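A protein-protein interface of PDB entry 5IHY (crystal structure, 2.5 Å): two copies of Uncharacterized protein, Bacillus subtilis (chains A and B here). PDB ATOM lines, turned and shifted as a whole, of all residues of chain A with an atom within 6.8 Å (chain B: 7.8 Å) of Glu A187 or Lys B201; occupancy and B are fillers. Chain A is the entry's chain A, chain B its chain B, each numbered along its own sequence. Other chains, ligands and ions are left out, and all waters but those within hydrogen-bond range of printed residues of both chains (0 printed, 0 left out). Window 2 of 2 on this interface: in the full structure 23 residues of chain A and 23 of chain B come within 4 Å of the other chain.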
ATOM      1  N   GLY A 136     -17.698 -13.195  -8.000  1.00  0.00           N
ATOM      2  CA  GLY A 136     -16.477 -13.209  -8.815  1.00  0.00           C
ATOM      3  C   GLY A 136     -15.200 -12.949  -8.024  1.00  0.00           C
ATOM      4  O   GLY A 136     -15.165 -13.088  -6.797  1.00  0.00           O
ATOM      5  N   ILE A 173     -26.749 -15.040  -7.519  1.00  0.00           N
ATOM      6  CA  ILE A 173     -27.118 -15.161  -8.934  1.00  0.00           C
ATOM      7  C   ILE A 173     -28.604 -15.496  -9.171  1.00  0.00           C
ATOM      8  O   ILE A 173     -29.127 -15.232 -10.253  1.00  0.00           O
ATOM      9  CB  ILE A 173     -26.183 -16.151  -9.697  1.00  0.00           C
ATOM     10  CG1 ILE A 173     -26.403 -16.051 -11.215  1.00  0.00           C
ATOM     11  CG2 ILE A 173     -26.344 -17.582  -9.167  1.00  0.00           C
ATOM     12  CD1 ILE A 173     -25.425 -16.857 -12.054  1.00  0.00           C
ATOM     13  N   ARG A 182     -27.916 -10.724 -14.939  1.00  0.00           N
ATOM     14  CA  ARG A 182     -27.896 -12.186 -14.895  1.00  0.00           C
ATOM     15  C   ARG A 182     -26.816 -12.773 -15.811  1.00  0.00           C
ATOM     16  O   ARG A 182     -26.019 -13.604 -15.367  1.00  0.00           O
ATOM     17  CB  ARG A 182     -29.274 -12.758 -15.238  1.00  0.00           C
ATOM     18  CG  ARG A 182     -29.549 -14.119 -14.626  1.00  0.00           C
ATOM     19  CD  ARG A 182     -30.957 -14.629 -14.969  1.00  0.00           C
ATOM     20  NE  ARG A 182     -31.986 -14.016 -14.127  1.00  0.00           N
ATOM     21  CZ  ARG A 182     -32.871 -13.110 -14.538  1.00  0.00           C
ATOM     22  NH1 ARG A 182     -32.889 -12.699 -15.802  1.00  0.00           N
ATOM     23  NH2 ARG A 182     -33.751 -12.619 -13.676  1.00  0.00           N
ATOM     24  N   GLU A 183     -26.785 -12.322 -17.070  1.00  0.00           N
ATOM     25  CA  GLU A 183     -25.759 -12.728 -18.046  1.00  0.00           C
ATOM     26  C   GLU A 183     -24.343 -12.400 -17.552  1.00  0.00           C
ATOM     27  O   GLU A 183     -23.440 -13.225 -17.680  1.00  0.00           O
ATOM     28  CB  GLU A 183     -26.001 -12.091 -19.426  1.00  0.00           C
ATOM     29  CG  GLU A 183     -27.300 -12.509 -20.113  1.00  0.00           C
ATOM     30  CD  GLU A 183     -27.480 -11.876 -21.493  1.00  0.00           C
ATOM     31  OE1 GLU A 183     -28.360 -10.991 -21.655  1.00  0.00           O
ATOM     32  OE2 GLU A 183     -26.734 -12.264 -22.420  1.00  0.00           O
ATOM     33  N   LEU A 184     -24.164 -11.205 -16.984  1.00  0.00           N
ATOM     34  CA  LEU A 184     -22.892 -10.799 -16.372  1.00  0.00           C
ATOM     35  C   LEU A 184     -22.534 -11.607 -15.124  1.00  0.00           C
ATOM     36  O   LEU A 184     -21.354 -11.807 -14.828  1.00  0.00           O
ATOM     37  CB  LEU A 184     -22.910  -9.317 -16.001  1.00  0.00           C
ATOM     38  CG  LEU A 184     -23.001  -8.233 -17.075  1.00  0.00           C
ATOM     39  CD1 LEU A 184     -22.878  -6.871 -16.403  1.00  0.00           C
ATOM     40  CD2 LEU A 184     -21.940  -8.392 -18.158  1.00  0.00           C
ATOM     41  N   ALA A 185     -23.550 -12.049 -14.387  1.00  0.00           N
ATOM     42  CA  ALA A 185     -23.349 -12.850 -13.182  1.00  0.00           C
ATOM     43  C   ALA A 185     -22.856 -14.264 -13.490  1.00  0.00           C
ATOM     44  O   ALA A 185     -22.147 -14.857 -12.679  1.00  0.00           O
ATOM     45  CB  ALA A 185     -24.619 -12.899 -12.360  1.00  0.00           C
ATOM     46  N   GLU A 186     -23.218 -14.788 -14.663  1.00  0.00           N
ATOM     47  CA  GLU A 186     -22.877 -16.163 -15.046  1.00  0.00           C
ATOM     48  C   GLU A 186     -21.383 -16.430 -14.923  1.00  0.00           C
ATOM     49  O   GLU A 186     -20.964 -17.376 -14.252  1.00  0.00           O
ATOM     50  CB  GLU A 186     -23.337 -16.475 -16.474  1.00  0.00           C
ATOM     51  CG  GLU A 186     -24.841 -16.316 -16.713  1.00  0.00           C
ATOM     52  CD  GLU A 186     -25.664 -17.558 -16.353  1.00  0.00           C
ATOM     53  OE1 GLU A 186     -25.146 -18.695 -16.475  1.00  0.00           O
ATOM     54  OE2 GLU A 186     -26.846 -17.387 -15.968  1.00  0.00           O
ATOM     55  N   GLU A 187     -20.587 -15.583 -15.569  1.00  0.00           N
ATOM     56  CA  GLU A 187     -19.148 -15.781 -15.621  1.00  0.00           C
ATOM     57  C   GLU A 187     -18.483 -15.552 -14.258  1.00  0.00           C
ATOM     58  O   GLU A 187     -17.490 -16.203 -13.940  1.00  0.00           O
ATOM     59  CB  GLU A 187     -18.519 -14.899 -16.706  1.00  0.00           C
ATOM     60  CG  GLU A 187     -17.187 -15.441 -17.252  1.00  0.00           C
ATOM     61  CD  GLU A 187     -16.171 -14.340 -17.591  1.00  0.00           C
ATOM     62  OE1 GLU A 187     -16.570 -13.275 -18.115  1.00  0.00           O
ATOM     63  OE2 GLU A 187     -14.961 -14.548 -17.331  1.00  0.00           O
ATOM     64  N   ARG A 188     -19.038 -14.637 -13.462  1.00  0.00           N
ATOM     65  CA  ARG A 188     -18.503 -14.319 -12.132  1.00  0.00           C
ATOM     66  C   ARG A 188     -18.803 -15.433 -11.148  1.00  0.00           C
ATOM     67  O   ARG A 188     -17.951 -15.810 -10.347  1.00  0.00           O
ATOM     68  CB  ARG A 188     -19.064 -12.992 -11.604  1.00  0.00           C
ATOM     69  CG  ARG A 188     -18.612 -11.770 -12.389  1.00  0.00           C
ATOM     70  CD  ARG A 188     -18.907 -10.488 -11.637  1.00  0.00           C
ATOM     71  NE  ARG A 188     -18.533  -9.313 -12.420  1.00  0.00           N
ATOM     72  CZ  ARG A 188     -18.253  -8.115 -11.905  1.00  0.00           C
ATOM     73  NH1 ARG A 188     -18.301  -7.908 -10.594  1.00  0.00           N
ATOM     74  NH2 ARG A 188     -17.917  -7.122 -12.703  1.00  0.00           N
ATOM     75  N   HIS A 189     -20.021 -15.960 -11.225  1.00  0.00           N
ATOM     76  CA  HIS A 189     -20.455 -17.053 -10.371  1.00  0.00           C
ATOM     77  C   HIS A 189     -19.629 -18.320 -10.603  1.00  0.00           C
ATOM     78  O   HIS A 189     -19.269 -19.019  -9.644  1.00  0.00           O
ATOM     79  CB  HIS A 189     -21.942 -17.322 -10.587  1.00  0.00           C
ATOM     80  CG  HIS A 189     -22.484 -18.434  -9.750  1.00  0.00           C
ATOM     81  ND1 HIS A 189     -22.860 -18.259  -8.437  1.00  0.00           N
ATOM     82  CD2 HIS A 189     -22.716 -19.737 -10.039  1.00  0.00           C
ATOM     83  CE1 HIS A 189     -23.308 -19.405  -7.954  1.00  0.00           C
ATOM     84  NE2 HIS A 189     -23.229 -20.318  -8.905  1.00  0.00           N
ATOM     85  N   GLU A 190     -19.320 -18.599 -11.868  1.00  0.00           N
ATOM     86  CA  GLU A 190     -18.555 -19.797 -12.229  1.00  0.00           C
ATOM     87  C   GLU A 190     -17.116 -19.712 -11.753  1.00  0.00           C
ATOM     88  O   GLU A 190     -16.564 -20.711 -11.273  1.00  0.00           O
ATOM     89  CB  GLU A 190     -18.607 -20.078 -13.737  1.00  0.00           C
ATOM     90  CG  GLU A 190     -19.925 -20.683 -14.208  1.00  0.00           C
ATOM     91  CD  GLU A 190     -20.242 -22.037 -13.556  1.00  0.00           C
ATOM     92  OE1 GLU A 190     -19.294 -22.790 -13.199  1.00  0.00           O
ATOM     93  OE2 GLU A 190     -21.450 -22.349 -13.408  1.00  0.00           O
ATOM     94  N   PHE A 191     -16.515 -18.526 -11.873  1.00  0.00           N
ATOM     95  CA  PHE A 191     -15.163 -18.316 -11.366  1.00  0.00           C
ATOM     96  C   PHE A 191     -15.112 -18.538  -9.857  1.00  0.00           C
ATOM     97  O   PHE A 191     -14.166 -19.129  -9.345  1.00  0.00           O
ATOM     98  CB  PHE A 191     -14.603 -16.934 -11.708  1.00  0.00           C
ATOM     99  CG  PHE A 191     -13.233 -16.701 -11.129  1.00  0.00           C
ATOM    100  CD1 PHE A 191     -12.101 -17.163 -11.790  1.00  0.00           C
ATOM    101  CD2 PHE A 191     -13.081 -16.094  -9.891  1.00  0.00           C
ATOM    102  CE1 PHE A 191     -10.841 -16.986 -11.245  1.00  0.00           C
ATOM    103  CE2 PHE A 191     -11.814 -15.914  -9.335  1.00  0.00           C
ATOM    104  CZ  PHE A 191     -10.696 -16.358 -10.015  1.00  0.00           C
ATOM    105  N   MET A 192     -16.136 -18.056  -9.160  1.00  0.00           N
ATOM    106  CA  MET A 192     -16.277 -18.277  -7.723  1.00  0.00           C
ATOM    107  C   MET A 192     -16.334 -19.780  -7.379  1.00  0.00           C
ATOM    108  O   MET A 192     -15.689 -20.226  -6.429  1.00  0.00           O
ATOM    109  CB  MET A 192     -17.503 -17.524  -7.199  1.00  0.00           C
ATOM    110  CG  MET A 192     -17.526 -17.303  -5.695  1.00  0.00           C
ATOM    111  SD  MET A 192     -18.717 -15.859  -5.117  1.00  0.00           S
ATOM    112  CE  MET A 192     -20.366 -16.424  -5.975  1.00  0.00           C
ATOM    113  N   TYR B 195      -6.525 -15.843 -11.213  1.00  0.00           N
ATOM    114  CA  TYR B 195      -7.253 -14.958 -10.307  1.00  0.00           C
ATOM    115  C   TYR B 195      -6.976 -13.488 -10.621  1.00  0.00           C
ATOM    116  O   TYR B 195      -7.907 -12.705 -10.747  1.00  0.00           O
ATOM    117  CB  TYR B 195      -6.961 -15.262  -8.824  1.00  0.00           C
ATOM    118  CG  TYR B 195      -7.674 -14.304  -7.898  1.00  0.00           C
ATOM    119  CD1 TYR B 195      -7.066 -13.112  -7.484  1.00  0.00           C
ATOM    120  CD2 TYR B 195      -8.971 -14.572  -7.452  1.00  0.00           C
ATOM    121  CE1 TYR B 195      -7.733 -12.214  -6.642  1.00  0.00           C
ATOM    122  CE2 TYR B 195      -9.647 -13.678  -6.610  1.00  0.00           C
ATOM    123  CZ  TYR B 195      -9.025 -12.502  -6.214  1.00  0.00           C
ATOM    124  OH  TYR B 195      -9.692 -11.620  -5.386  1.00  0.00           O
ATOM    125  N   ILE B 196      -5.709 -13.115 -10.748  1.00  0.00           N
ATOM    126  CA  ILE B 196      -5.359 -11.737 -11.111  1.00  0.00           C
ATOM    127  C   ILE B 196      -6.026 -11.313 -12.424  1.00  0.00           C
ATOM    128  O   ILE B 196      -6.590 -10.221 -12.514  1.00  0.00           O
ATOM    129  CB  ILE B 196      -3.826 -11.518 -11.179  1.00  0.00           C
ATOM    130  CG1 ILE B 196      -3.236 -11.493  -9.765  1.00  0.00           C
ATOM    131  CG2 ILE B 196      -3.489 -10.219 -11.913  1.00  0.00           C
ATOM    132  CD1 ILE B 196      -1.770 -11.886  -9.706  1.00  0.00           C
ATOM    133  N   ARG B 197      -5.968 -12.189 -13.424  1.00  0.00           N
ATOM    134  CA  ARG B 197      -6.641 -11.982 -14.703  1.00  0.00           C
ATOM    135  C   ARG B 197      -8.139 -11.685 -14.544  1.00  0.00           C
ATOM    136  O   ARG B 197      -8.651 -10.711 -15.099  1.00  0.00           O
ATOM    137  CB  ARG B 197      -6.430 -13.211 -15.585  1.00  0.00           C
ATOM    138  CG  ARG B 197      -6.550 -12.945 -17.050  1.00  0.00           C
ATOM    139  CD  ARG B 197      -5.558 -13.801 -17.831  1.00  0.00           C
ATOM    140  NE  ARG B 197      -5.948 -13.893 -19.236  1.00  0.00           N
ATOM    141  CZ  ARG B 197      -6.750 -14.832 -19.730  1.00  0.00           C
ATOM    142  NH1 ARG B 197      -7.249 -15.780 -18.938  1.00  0.00           N
ATOM    143  NH2 ARG B 197      -7.051 -14.826 -21.025  1.00  0.00           N
ATOM    144  N   GLN B 198      -8.826 -12.522 -13.770  1.00  0.00           N
ATOM    145  CA  GLN B 198     -10.257 -12.344 -13.490  1.00  0.00           C
ATOM    146  C   GLN B 198     -10.546 -11.033 -12.748  1.00  0.00           C
ATOM    147  O   GLN B 198     -11.548 -10.363 -13.017  1.00  0.00           O
ATOM    148  CB  GLN B 198     -10.792 -13.537 -12.688  1.00  0.00           C
ATOM    149  CG  GLN B 198     -12.285 -13.531 -12.471  1.00  0.00           C
ATOM    150  CD  GLN B 198     -13.083 -13.724 -13.751  1.00  0.00           C
ATOM    151  OE1 GLN B 198     -12.690 -14.483 -14.640  1.00  0.00           O
ATOM    152  NE2 GLN B 198     -14.220 -13.042 -13.841  1.00  0.00           N
ATOM    153  N   LEU B 199      -9.661 -10.677 -11.820  1.00  0.00           N
ATOM    154  CA  LEU B 199      -9.775  -9.438 -11.058  1.00  0.00           C
ATOM    155  C   LEU B 199      -9.651  -8.206 -11.960  1.00  0.00           C
ATOM    156  O   LEU B 199     -10.367  -7.224 -11.780  1.00  0.00           O
ATOM    157  CB  LEU B 199      -8.726  -9.410  -9.940  1.00  0.00           C
ATOM    158  CG  LEU B 199      -8.876  -8.425  -8.772  1.00  0.00           C
ATOM    159  CD1 LEU B 199     -10.167  -8.639  -7.984  1.00  0.00           C
ATOM    160  CD2 LEU B 199      -7.664  -8.516  -7.841  1.00  0.00           C
ATOM    161  N   GLU B 200      -8.757  -8.283 -12.943  1.00  0.00           N
ATOM    162  CA  GLU B 200      -8.512  -7.182 -13.867  1.00  0.00           C
ATOM    163  C   GLU B 200      -9.696  -6.892 -14.784  1.00  0.00           C
ATOM    164  O   GLU B 200      -9.833  -5.773 -15.272  1.00  0.00           O
ATOM    165  CB  GLU B 200      -7.246  -7.425 -14.689  1.00  0.00           C
ATOM    166  CG  GLU B 200      -5.962  -7.233 -13.884  1.00  0.00           C
ATOM    167  CD  GLU B 200      -4.715  -7.726 -14.601  1.00  0.00           C
ATOM    168  OE1 GLU B 200      -4.778  -8.765 -15.305  1.00  0.00           O
ATOM    169  OE2 GLU B 200      -3.659  -7.076 -14.445  1.00  0.00           O
ATOM    170  N   LYS B 201     -10.554  -7.877 -15.018  1.00  0.00           N
ATOM    171  CA  LYS B 201     -11.748  -7.590 -15.799  1.00  0.00           C
ATOM    172  C   LYS B 201     -12.993  -7.331 -14.935  1.00  0.00           C
ATOM    173  O   LYS B 201     -13.930  -6.663 -15.385  1.00  0.00           O
ATOM    174  CB  LYS B 201     -11.964  -8.610 -16.926  1.00  0.00           C
ATOM    175  CG  LYS B 201     -12.518  -9.950 -16.547  1.00  0.00           C
ATOM    176  CD  LYS B 201     -12.362 -10.898 -17.734  1.00  0.00           C
ATOM    177  CE  LYS B 201     -13.435 -11.969 -17.731  1.00  0.00           C
ATOM    178  NZ  LYS B 201     -14.819 -11.393 -17.817  1.00  0.00           N
ATOM    179  N   ASP B 202     -12.972  -7.825 -13.695  1.00  0.00           N
ATOM    180  CA  ASP B 202     -13.939  -7.435 -12.661  1.00  0.00           C
ATOM    181  C   ASP B 202     -13.789  -5.956 -12.280  1.00  0.00           C
ATOM    182  O   ASP B 202     -14.771  -5.286 -11.950  1.00  0.00           O
ATOM    183  CB  ASP B 202     -13.744  -8.281 -11.393  1.00  0.00           C
ATOM    184  CG  ASP B 202     -14.379  -9.671 -11.489  1.00  0.00           C
ATOM    185  OD1 ASP B 202     -14.627 -10.169 -12.605  1.00  0.00           O
ATOM    186  OD2 ASP B 202     -14.622 -10.279 -10.425  1.00  0.00           O
ATOM    187  N   ILE B 203     -12.549  -5.468 -12.311  1.00  0.00           N
ATOM    188  CA  ILE B 203     -12.213  -4.087 -11.971  1.00  0.00           C
ATOM    189  C   ILE B 203     -11.397  -3.479 -13.116  1.00  0.00           C
ATOM    190  O   ILE B 203     -10.163  -3.506 -13.080  1.00  0.00           O
ATOM    191  CB  ILE B 203     -11.398  -4.011 -10.646  1.00  0.00           C
ATOM    192  CG1 ILE B 203     -12.093  -4.813  -9.537  1.00  0.00           C
ATOM    193  CG2 ILE B 203     -11.165  -2.557 -10.227  1.00  0.00           C
ATOM    194  CD1 ILE B 203     -11.295  -4.966  -8.266  1.00  0.00           C
ATOM    195  N   PRO B 204     -12.079  -2.949 -14.153  1.00  0.00           N
ATOM    196  CA  PRO B 204     -11.354  -2.300 -15.251  1.00  0.00           C
ATOM    197  C   PRO B 204     -10.574  -1.079 -14.765  1.00  0.00           C
ATOM    198  O   PRO B 204     -11.134  -0.225 -14.078  1.00  0.00           O
ATOM    199  CB  PRO B 204     -12.469  -1.890 -16.229  1.00  0.00           C
ATOM    200  CG  PRO B 204     -13.740  -1.981 -15.459  1.00  0.00           C
ATOM    201  CD  PRO B 204     -13.529  -3.030 -14.423  1.00  0.00           C
ATOM    202  N   GLY B 205      -9.288  -1.020 -15.097  1.00  0.00           N
ATOM    203  CA  GLY B 205      -8.418   0.069 -14.638  1.00  0.00           C
ATOM    204  C   GLY B 205      -7.793  -0.126 -13.261  1.00  0.00           C
ATOM    205  O   GLY B 205      -7.234   0.819 -12.695  1.00  0.00           O
ATOM    206  N   ILE B 206      -7.874  -1.341 -12.716  1.00  0.00           N
ATOM    207  CA  ILE B 206      -7.246  -1.668 -11.428  1.00  0.00           C
ATOM    208  C   ILE B 206      -5.748  -1.373 -11.445  1.00  0.00           C
ATOM    209  O   ILE B 206      -5.180  -0.922 -10.441  1.00  0.00           O
ATOM    210  CB  ILE B 206      -7.493  -3.146 -11.015  1.00  0.00           C
ATOM    211  CG1 ILE B 206      -7.020  -3.398  -9.578  1.00  0.00           C
ATOM    212  CG2 ILE B 206      -6.842  -4.125 -12.017  1.00  0.00           C
ATOM    213  CD1 ILE B 206      -7.342  -4.791  -9.047  1.00  0.00           C
ATOM    214  N   ASP B 207      -5.115  -1.625 -12.589  1.00  0.00           N
ATOM    215  CA  ASP B 207      -3.703  -1.302 -12.777  1.00  0.00           C
ATOM    216  C   ASP B 207      -3.570   0.161 -13.174  1.00  0.00           C
ATOM    217  O   ASP B 207      -2.634   0.831 -12.754  1.00  0.00           O
ATOM    218  CB  ASP B 207      -3.058  -2.200 -13.843  1.00  0.00           C
ATOM    219  CG  ASP B 207      -3.368  -3.682 -13.641  1.00  0.00           C
ATOM    220  OD1 ASP B 207      -2.852  -4.291 -12.675  1.00  0.00           O
ATOM    221  OD2 ASP B 207      -4.120  -4.237 -14.473  1.00  0.00           O
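Printed residues of chain A that touch a printed residue of chain B: Gly A136, Glu A187, Arg A188 and Phe A191. Hydrophobic or aromatic side chains of chain A within 4 Å of the printed part of chain B: Phe A191. Among the printed residues, Asp or Glu carboxylates within 4 Å of a Lys or Arg side-chain nitrogen of the other chain: Glu A187 with Lys B201.
Leu A184 touches none of the printed residues of chain B. Glu A187 touches just these residues of chain B: Gln B198 (3.5 Å) and Lys B201 (2.6 Å). Printed residues of chain B within 4 Å of Arg A188: Asp B202 (3.7 Å). Of the printed residues of chain B, Phe A191 touches Tyr B195 and Gln B198. Printed residues of chain A within 4 Å of Tyr B195: Phe A191. Printed residues of chain A within 4 Å of Gln B198: Glu A187 (3.5 Å) and Phe A191 (3.6 Å). Of chain A, only Glu A187 (2.6 Å) comes within 4 Å of Lys B201. The nearest printed residue of chain B that does not touch Phe A191 is Ile B196 (6.0 Å).
Asp B202 touches Gly A136 (OD2 to C, 3.6 Å). Glu A187 touches Gln B198. Asp B202 touches Arg A188 (O to NH2, 3.7 Å). Phe A191 touches Tyr B195 (CZ to CD2, 3.6 Å). Phe A191 touches Gln B198 (CG to CG, 3.6 Å).
The side-chain carboxylate of Glu A187 is in salt-bridge range of the side-chain amino group of Lys B201 (2.6 Å).
No position is printed for both chains. Of the 6 pairs that touch across the chains among the printed residues, none has its exchanged pair printed and touching as well.
The side-chain amide nitrogen (NE2) of Gln B198 is in hydrogen-bond range of the side-chain carboxylate (OD1) of Asp B202 (3.2 Å).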
